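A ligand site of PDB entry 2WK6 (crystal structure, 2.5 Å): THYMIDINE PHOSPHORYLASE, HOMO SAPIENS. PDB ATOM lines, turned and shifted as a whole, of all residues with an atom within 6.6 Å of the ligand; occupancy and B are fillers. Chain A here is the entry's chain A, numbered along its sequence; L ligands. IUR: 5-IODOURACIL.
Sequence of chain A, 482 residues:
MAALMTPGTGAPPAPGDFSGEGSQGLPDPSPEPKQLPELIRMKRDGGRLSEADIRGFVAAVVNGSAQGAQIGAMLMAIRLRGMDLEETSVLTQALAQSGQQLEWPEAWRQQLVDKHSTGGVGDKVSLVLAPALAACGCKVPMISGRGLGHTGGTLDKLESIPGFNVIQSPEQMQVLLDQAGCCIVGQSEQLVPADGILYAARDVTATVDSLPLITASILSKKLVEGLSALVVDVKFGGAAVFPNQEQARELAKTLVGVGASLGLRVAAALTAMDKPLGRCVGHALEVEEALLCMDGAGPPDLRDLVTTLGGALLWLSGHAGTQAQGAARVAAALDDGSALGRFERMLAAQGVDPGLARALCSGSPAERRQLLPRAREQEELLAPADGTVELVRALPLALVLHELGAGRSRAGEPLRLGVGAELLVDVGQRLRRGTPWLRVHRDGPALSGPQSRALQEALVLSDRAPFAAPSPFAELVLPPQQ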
ATOM      1  N   HIS A 116     -27.864  22.870  -7.389  1.00  0.00           N
ATOM      2  CA  HIS A 116     -26.614  22.498  -7.990  1.00  0.00           C
ATOM      3  C   HIS A 116     -25.796  21.780  -6.942  1.00  0.00           C
ATOM      4  O   HIS A 116     -25.891  22.101  -5.761  1.00  0.00           O
ATOM      5  CB  HIS A 116     -25.860  23.740  -8.461  1.00  0.00           C
ATOM      6  CG  HIS A 116     -24.897  23.484  -9.580  1.00  0.00           C
ATOM      7  ND1 HIS A 116     -25.285  23.462 -10.906  1.00  0.00           N
ATOM      8  CD2 HIS A 116     -23.572  23.183  -9.575  1.00  0.00           C
ATOM      9  CE1 HIS A 116     -24.251  23.156 -11.661  1.00  0.00           C
ATOM     10  NE2 HIS A 116     -23.195  22.979 -10.883  1.00  0.00           N
ATOM     11  N   SER A 117     -25.021  20.787  -7.371  1.00  0.00           N
ATOM     12  CA  SER A 117     -24.173  20.025  -6.460  1.00  0.00           C
ATOM     13  C   SER A 117     -22.737  20.335  -6.807  1.00  0.00           C
ATOM     14  O   SER A 117     -22.401  20.459  -7.975  1.00  0.00           O
ATOM     15  CB  SER A 117     -24.422  18.530  -6.624  1.00  0.00           C
ATOM     16  OG  SER A 117     -23.403  17.768  -5.982  1.00  0.00           O
ATOM     17  N   THR A 118     -21.875  20.465  -5.797  1.00  0.00           N
ATOM     18  CA  THR A 118     -20.467  20.728  -6.100  1.00  0.00           C
ATOM     19  C   THR A 118     -19.825  19.491  -6.701  1.00  0.00           C
ATOM     20  O   THR A 118     -18.683  19.542  -7.160  1.00  0.00           O
ATOM     21  CB  THR A 118     -19.671  21.146  -4.845  1.00  0.00           C
ATOM     22  OG1 THR A 118     -19.749  20.111  -3.849  1.00  0.00           O
ATOM     23  CG2 THR A 118     -20.217  22.465  -4.299  1.00  0.00           C
ATOM     24  N   GLY A 119     -20.546  18.364  -6.701  1.00  0.00           N
ATOM     25  CA  GLY A 119     -20.007  17.160  -7.292  1.00  0.00           C
ATOM     26  C   GLY A 119     -19.607  16.046  -6.338  1.00  0.00           C
ATOM     27  O   GLY A 119     -19.078  16.272  -5.240  1.00  0.00           O
ATOM     28  N   ILE A 143     -28.745  24.353 -15.860  1.00  0.00           N
ATOM     29  CA  ILE A 143     -27.539  24.347 -16.657  1.00  0.00           C
ATOM     30  C   ILE A 143     -26.536  23.691 -15.725  1.00  0.00           C
ATOM     31  O   ILE A 143     -26.193  24.260 -14.684  1.00  0.00           O
ATOM     32  CB  ILE A 143     -27.031  25.774 -16.961  1.00  0.00           C
ATOM     33  CG1 ILE A 143     -28.154  26.625 -17.549  1.00  0.00           C
ATOM     34  CG2 ILE A 143     -25.857  25.703 -17.939  1.00  0.00           C
ATOM     35  CD1 ILE A 143     -27.885  28.120 -17.556  1.00  0.00           C
ATOM     36  N   SER A 144     -26.102  22.474 -16.031  1.00  0.00           N
ATOM     37  CA  SER A 144     -25.118  21.816 -15.177  1.00  0.00           C
ATOM     38  C   SER A 144     -23.865  21.579 -15.994  1.00  0.00           C
ATOM     39  O   SER A 144     -23.622  22.266 -16.970  1.00  0.00           O
ATOM     40  CB  SER A 144     -25.654  20.493 -14.590  1.00  0.00           C
ATOM     41  OG  SER A 144     -26.018  19.582 -15.609  1.00  0.00           O
ATOM     42  N   GLY A 145     -23.061  20.609 -15.593  1.00  0.00           N
ATOM     43  CA  GLY A 145     -21.841  20.349 -16.337  1.00  0.00           C
ATOM     44  C   GLY A 145     -21.509  18.891 -16.480  1.00  0.00           C
ATOM     45  O   GLY A 145     -22.283  18.004 -16.064  1.00  0.00           O
ATOM     46  N   LEU A 148     -16.046  16.413 -13.360  1.00  0.00           N
ATOM     47  CA  LEU A 148     -14.982  17.305 -12.932  1.00  0.00           C
ATOM     48  C   LEU A 148     -14.054  16.517 -12.036  1.00  0.00           C
ATOM     49  O   LEU A 148     -14.399  16.175 -10.908  1.00  0.00           O
ATOM     50  CB  LEU A 148     -15.595  18.482 -12.184  1.00  0.00           C
ATOM     51  CG  LEU A 148     -15.152  19.912 -12.503  1.00  0.00           C
ATOM     52  CD1 LEU A 148     -15.029  20.140 -14.008  1.00  0.00           C
ATOM     53  CD2 LEU A 148     -16.180  20.858 -11.893  1.00  0.00           C
ATOM     54  N   THR A 151     -15.194  13.365  -9.851  1.00  0.00           N
ATOM     55  CA  THR A 151     -16.647  13.406  -9.674  1.00  0.00           C
ATOM     56  C   THR A 151     -17.401  13.275 -11.000  1.00  0.00           C
ATOM     57  O   THR A 151     -16.873  13.610 -12.057  1.00  0.00           O
ATOM     58  CB  THR A 151     -17.113  14.704  -8.937  1.00  0.00           C
ATOM     59  OG1 THR A 151     -16.990  15.838  -9.812  1.00  0.00           O
ATOM     60  CG2 THR A 151     -16.282  14.951  -7.697  1.00  0.00           C
ATOM     61  N   GLN A 187     -23.219  24.113 -20.755  1.00  0.00           N
ATOM     62  CA  GLN A 187     -22.641  25.362 -21.227  1.00  0.00           C
ATOM     63  C   GLN A 187     -22.549  25.272 -22.752  1.00  0.00           C
ATOM     64  O   GLN A 187     -22.360  24.186 -23.318  1.00  0.00           O
ATOM     65  CB  GLN A 187     -21.248  25.573 -20.637  1.00  0.00           C
ATOM     66  CG  GLN A 187     -21.191  25.511 -19.126  1.00  0.00           C
ATOM     67  CD  GLN A 187     -20.635  24.181 -18.624  1.00  0.00           C
ATOM     68  OE1 GLN A 187     -20.971  23.100 -19.148  1.00  0.00           O
ATOM     69  NE2 GLN A 187     -19.785  24.243 -17.591  1.00  0.00           N
ATOM     70  N   ASP A 195     -17.337  29.754 -19.003  1.00  0.00           N
ATOM     71  CA  ASP A 195     -17.261  28.689 -18.018  1.00  0.00           C
ATOM     72  C   ASP A 195     -17.122  27.331 -18.711  1.00  0.00           C
ATOM     73  O   ASP A 195     -16.403  26.456 -18.219  1.00  0.00           O
ATOM     74  CB  ASP A 195     -18.501  28.696 -17.109  1.00  0.00           C
ATOM     75  CG  ASP A 195     -18.490  27.557 -16.109  1.00  0.00           C
ATOM     76  OD1 ASP A 195     -19.031  26.467 -16.416  1.00  0.00           O
ATOM     77  OD2 ASP A 195     -17.902  27.735 -15.030  1.00  0.00           O
ATOM     78  N   TYR A 199     -14.180  25.148 -17.436  1.00  0.00           N
ATOM     79  CA  TYR A 199     -14.655  23.953 -16.747  1.00  0.00           C
ATOM     80  C   TYR A 199     -13.946  22.724 -17.324  1.00  0.00           C
ATOM     81  O   TYR A 199     -13.407  21.896 -16.589  1.00  0.00           O
ATOM     82  CB  TYR A 199     -16.167  23.851 -16.961  1.00  0.00           C
ATOM     83  CG  TYR A 199     -16.914  22.799 -16.176  1.00  0.00           C
ATOM     84  CD1 TYR A 199     -16.797  21.444 -16.499  1.00  0.00           C
ATOM     85  CD2 TYR A 199     -17.805  23.169 -15.163  1.00  0.00           C
ATOM     86  CE1 TYR A 199     -17.568  20.477 -15.834  1.00  0.00           C
ATOM     87  CE2 TYR A 199     -18.565  22.223 -14.493  1.00  0.00           C
ATOM     88  CZ  TYR A 199     -18.451  20.877 -14.828  1.00  0.00           C
ATOM     89  OH  TYR A 199     -19.215  19.949 -14.170  1.00  0.00           O
ATOM     90  N   ARG A 202     -10.245  22.873 -16.376  1.00  0.00           N
ATOM     91  CA  ARG A 202     -10.067  22.618 -14.950  1.00  0.00           C
ATOM     92  C   ARG A 202     -10.126  21.137 -14.632  1.00  0.00           C
ATOM     93  O   ARG A 202      -9.322  20.608 -13.857  1.00  0.00           O
ATOM     94  CB  ARG A 202     -11.135  23.335 -14.130  1.00  0.00           C
ATOM     95  CG  ARG A 202     -10.853  24.812 -13.879  1.00  0.00           C
ATOM     96  CD  ARG A 202     -12.090  25.487 -13.293  1.00  0.00           C
ATOM     97  NE  ARG A 202     -12.432  24.945 -11.982  1.00  0.00           N
ATOM     98  CZ  ARG A 202     -13.665  24.805 -11.531  1.00  0.00           C
ATOM     99  NH1 ARG A 202     -14.696  25.156 -12.298  1.00  0.00           N
ATOM    100  NH2 ARG A 202     -13.889  24.301 -10.315  1.00  0.00           N
ATOM    101  N   VAL A 208      -9.646  21.939 -10.324  1.00  0.00           N
ATOM    102  CA  VAL A 208     -11.050  21.865  -9.966  1.00  0.00           C
ATOM    103  C   VAL A 208     -11.291  22.442  -8.578  1.00  0.00           C
ATOM    104  O   VAL A 208     -12.150  23.298  -8.390  1.00  0.00           O
ATOM    105  CB  VAL A 208     -11.553  20.414  -9.940  1.00  0.00           C
ATOM    106  CG1 VAL A 208     -12.970  20.359  -9.343  1.00  0.00           C
ATOM    107  CG2 VAL A 208     -11.521  19.830 -11.339  1.00  0.00           C
ATOM    108  N   ASP A 209     -10.504  21.975  -7.611  1.00  0.00           N
ATOM    109  CA  ASP A 209     -10.647  22.408  -6.226  1.00  0.00           C
ATOM    110  C   ASP A 209     -10.072  23.777  -5.894  1.00  0.00           C
ATOM    111  O   ASP A 209      -9.096  23.911  -5.171  1.00  0.00           O
ATOM    112  CB  ASP A 209     -10.059  21.335  -5.301  1.00  0.00           C
ATOM    113  CG  ASP A 209      -8.575  21.083  -5.560  1.00  0.00           C
ATOM    114  OD1 ASP A 209      -8.106  21.270  -6.716  1.00  0.00           O
ATOM    115  OD2 ASP A 209      -7.886  20.669  -4.597  1.00  0.00           O
ATOM    116  N   SER A 210     -10.727  24.802  -6.432  1.00  0.00           N
ATOM    117  CA  SER A 210     -10.350  26.189  -6.232  1.00  0.00           C
ATOM    118  C   SER A 210     -11.622  26.936  -5.856  1.00  0.00           C
ATOM    119  O   SER A 210     -12.524  27.077  -6.687  1.00  0.00           O
ATOM    120  CB  SER A 210      -9.770  26.771  -7.533  1.00  0.00           C
ATOM    121  OG  SER A 210      -9.694  28.185  -7.503  1.00  0.00           O
ATOM    122  N   LEU A 213     -12.808  29.530  -8.337  1.00  0.00           N
ATOM    123  CA  LEU A 213     -13.177  28.976  -9.644  1.00  0.00           C
ATOM    124  C   LEU A 213     -14.480  28.200  -9.554  1.00  0.00           C
ATOM    125  O   LEU A 213     -15.284  28.206 -10.472  1.00  0.00           O
ATOM    126  CB  LEU A 213     -12.098  28.050 -10.208  1.00  0.00           C
ATOM    127  CG  LEU A 213     -10.785  28.692 -10.656  1.00  0.00           C
ATOM    128  CD1 LEU A 213      -9.823  27.589 -11.104  1.00  0.00           C
ATOM    129  CD2 LEU A 213     -11.048  29.704 -11.785  1.00  0.00           C
ATOM    130  N   ILE A 214     -14.678  27.503  -8.442  1.00  0.00           N
ATOM    131  CA  ILE A 214     -15.915  26.750  -8.287  1.00  0.00           C
ATOM    132  C   ILE A 214     -17.061  27.730  -8.151  1.00  0.00           C
ATOM    133  O   ILE A 214     -18.091  27.570  -8.805  1.00  0.00           O
ATOM    134  CB  ILE A 214     -15.863  25.837  -7.038  1.00  0.00           C
ATOM    135  CG1 ILE A 214     -14.751  24.801  -7.200  1.00  0.00           C
ATOM    136  CG2 ILE A 214     -17.216  25.151  -6.844  1.00  0.00           C
ATOM    137  CD1 ILE A 214     -14.360  24.060  -5.922  1.00  0.00           C
ATOM    138  N   THR A 215     -16.862  28.768  -7.318  1.00  0.00           N
ATOM    139  CA  THR A 215     -17.852  29.797  -7.040  1.00  0.00           C
ATOM    140  C   THR A 215     -18.328  30.536  -8.286  1.00  0.00           C
ATOM    141  O   THR A 215     -19.529  30.665  -8.535  1.00  0.00           O
ATOM    142  CB  THR A 215     -17.309  30.844  -6.021  1.00  0.00           C
ATOM    143  OG1 THR A 215     -16.953  30.185  -4.788  1.00  0.00           O
ATOM    144  CG2 THR A 215     -18.386  31.910  -5.716  1.00  0.00           C
ATOM    145  N   SER A 217     -17.834  29.584 -11.395  1.00  0.00           N
ATOM    146  CA  SER A 217     -18.364  28.591 -12.310  1.00  0.00           C
ATOM    147  C   SER A 217     -19.792  28.208 -11.985  1.00  0.00           C
ATOM    148  O   SER A 217     -20.658  28.164 -12.872  1.00  0.00           O
ATOM    149  CB  SER A 217     -17.505  27.327 -12.285  1.00  0.00           C
ATOM    150  OG  SER A 217     -18.014  26.367 -13.189  1.00  0.00           O
ATOM    151  N   ILE A 218     -20.043  27.932 -10.713  1.00  0.00           N
ATOM    152  CA  ILE A 218     -21.377  27.536 -10.305  1.00  0.00           C
ATOM    153  C   ILE A 218     -22.390  28.680 -10.390  1.00  0.00           C
ATOM    154  O   ILE A 218     -23.408  28.558 -11.073  1.00  0.00           O
ATOM    155  CB  ILE A 218     -21.369  26.955  -8.875  1.00  0.00           C
ATOM    156  CG1 ILE A 218     -20.607  25.629  -8.880  1.00  0.00           C
ATOM    157  CG2 ILE A 218     -22.811  26.787  -8.359  1.00  0.00           C
ATOM    158  CD1 ILE A 218     -20.392  24.987  -7.501  1.00  0.00           C
ATOM    159  N   LEU A 219     -22.109  29.786  -9.712  1.00  0.00           N
ATOM    160  CA  LEU A 219     -23.019  30.928  -9.718  1.00  0.00           C
ATOM    161  C   LEU A 219     -23.285  31.504 -11.106  1.00  0.00           C
ATOM    162  O   LEU A 219     -24.421  31.884 -11.416  1.00  0.00           O
ATOM    163  CB  LEU A 219     -22.500  32.033  -8.784  1.00  0.00           C
ATOM    164  CG  LEU A 219     -22.315  31.653  -7.311  1.00  0.00           C
ATOM    165  CD1 LEU A 219     -21.837  32.884  -6.562  1.00  0.00           C
ATOM    166  CD2 LEU A 219     -23.605  31.113  -6.707  1.00  0.00           C
ATOM    167  N   LYS A 221     -23.532  30.051 -13.882  1.00  0.00           N
ATOM    168  CA  LYS A 221     -24.543  29.235 -14.541  1.00  0.00           C
ATOM    169  C   LYS A 221     -25.910  29.601 -13.995  1.00  0.00           C
ATOM    170  O   LYS A 221     -26.842  29.839 -14.760  1.00  0.00           O
ATOM    171  CB  LYS A 221     -24.295  27.751 -14.276  1.00  0.00           C
ATOM    172  CG  LYS A 221     -23.045  27.202 -14.913  1.00  0.00           C
ATOM    173  CD  LYS A 221     -22.982  25.688 -14.776  1.00  0.00           C
ATOM    174  CE  LYS A 221     -21.579  25.225 -15.067  1.00  0.00           C
ATOM    175  NZ  LYS A 221     -20.654  25.924 -14.154  1.00  0.00           N
ATOM    176  N   LYS A 222     -26.009  29.635 -12.678  1.00  0.00           N
ATOM    177  CA  LYS A 222     -27.281  29.938 -12.052  1.00  0.00           C
ATOM    178  C   LYS A 222     -27.762  31.375 -12.224  1.00  0.00           C
ATOM    179  O   LYS A 222     -28.971  31.594 -12.318  1.00  0.00           O
ATOM    180  CB  LYS A 222     -27.237  29.559 -10.566  1.00  0.00           C
ATOM    181  CG  LYS A 222     -26.841  28.109 -10.362  1.00  0.00           C
ATOM    182  CD  LYS A 222     -27.664  27.216 -11.273  1.00  0.00           C
ATOM    183  CE  LYS A 222     -26.983  25.904 -11.520  1.00  0.00           C
ATOM    184  NZ  LYS A 222     -27.848  25.017 -12.349  1.00  0.00           N
ATOM    185  N   VAL A 241     -14.992  17.635  -3.467  1.00  0.00           N
ATOM    186  CA  VAL A 241     -13.981  18.509  -4.052  1.00  0.00           C
ATOM    187  C   VAL A 241     -13.124  18.984  -2.871  1.00  0.00           C
ATOM    188  O   VAL A 241     -11.886  19.019  -2.945  1.00  0.00           O
ATOM    189  CB  VAL A 241     -14.635  19.715  -4.761  1.00  0.00           C
ATOM    190  CG1 VAL A 241     -13.575  20.774  -5.114  1.00  0.00           C
ATOM    191  CG2 VAL A 241     -15.319  19.243  -6.035  1.00  0.00           C
ATOM    192  N   LEU A 251     -16.573  27.314   1.270  1.00  0.00           N
ATOM    193  CA  LEU A 251     -17.149  27.338  -0.059  1.00  0.00           C
ATOM    194  C   LEU A 251     -18.650  27.651   0.060  1.00  0.00           C
ATOM    195  O   LEU A 251     -19.192  28.504  -0.637  1.00  0.00           O
ATOM    196  CB  LEU A 251     -16.953  25.976  -0.733  1.00  0.00           C
ATOM    197  CG  LEU A 251     -16.925  25.952  -2.252  1.00  0.00           C
ATOM    198  CD1 LEU A 251     -17.260  24.563  -2.743  1.00  0.00           C
ATOM    199  CD2 LEU A 251     -17.911  26.951  -2.801  1.00  0.00           C
HETATM  200  N1  IUR L   1     -20.335  22.442 -10.632  1.00  0.00           N
HETATM  201  C2  IUR L   1     -20.029  23.543 -11.484  1.00  0.00           C
HETATM  202  O2  IUR L   1     -20.750  24.043 -12.306  1.00  0.00           O
HETATM  203  N3  IUR L   1     -18.718  24.072 -11.293  1.00  0.00           N
HETATM  204  C4  IUR L   1     -17.719  23.635 -10.380  1.00  0.00           C
HETATM  205  O4  IUR L   1     -16.632  24.199 -10.338  1.00  0.00           O
HETATM  206  C5  IUR L   1     -18.122  22.493  -9.551  1.00  0.00           C
HETATM  207  C6  IUR L   1     -19.412  21.941  -9.702  1.00  0.00           C
HETATM  208  I5  IUR L   1     -16.751  21.700  -8.158  1.00  0.00           I
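The guanidinium group (NH2) of Arg 202 is in hydrogen-bond range of an oxygen (O4) of the ligand, at 2.7 Å.
O2 of the ligand is in hydrogen-bond range of NZ of Lys 221, 2.6 Å away.
N1 of the ligand sits at hydrogen-bond distance from NE2 of His 116, 2.9 Å away.
The side-chain hydroxyl (OG) of Ser 217 sits at hydrogen-bond distance from a nitrogen (N3) of the ligand (3.1 Å).
NH2 of Arg 202 sits at hydrogen-bond distance from O of Val 208, at 2.8 Å.
The side-chain hydroxyl (OG) of Ser 117 lies close to the backbone NH (N) of Gly 119 (3.0 Å).
The backbone carbonyl oxygen (O) of Leu 148 is in hydrogen-bond range of the side-chain hydroxyl (OG1) of Thr 151, 2.8 Å away.
ND1 of His 116 lies close to NZ of Lys 222, at 3.3 Å.
The side-chain hydroxyl (OG) of Ser 217 lies close to the side-chain carboxylate (OD1) of Asp 195, 3.4 Å away.
The side-chain amino group (NZ) of Lys 221 lies within hydrogen-bond range of the backbone carbonyl oxygen (O) of Ser 217, 2.6 Å away.
NZ of Lys 221 lies within salt-bridge range of OD1 of Asp 195 (2.8 Å).
Residues that only touch the ligand: Thr 118 (3.1 Å), Ile 214 (3.4 Å), Ile 218 (3.4 Å), Leu 148 (3.5 Å), Val 241 (3.5 Å), Tyr 199 (3.6 Å) and Ser 117 (3.8 Å).
Hydrophobic or aromatic side chains that line the ligand: His 116, Leu 148, Tyr 199, Ile 214, Ile 218 and Val 241.
Within 4 Å of the ligand: His 116, Ser 117, Thr 118, Leu 148, Tyr 199, Arg 202, Ile 214, Ser 217, Ile 218, Lys 221 and Val 241.
The nearest printed residue that does not touch the ligand is Val 208 (4.2 Å).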
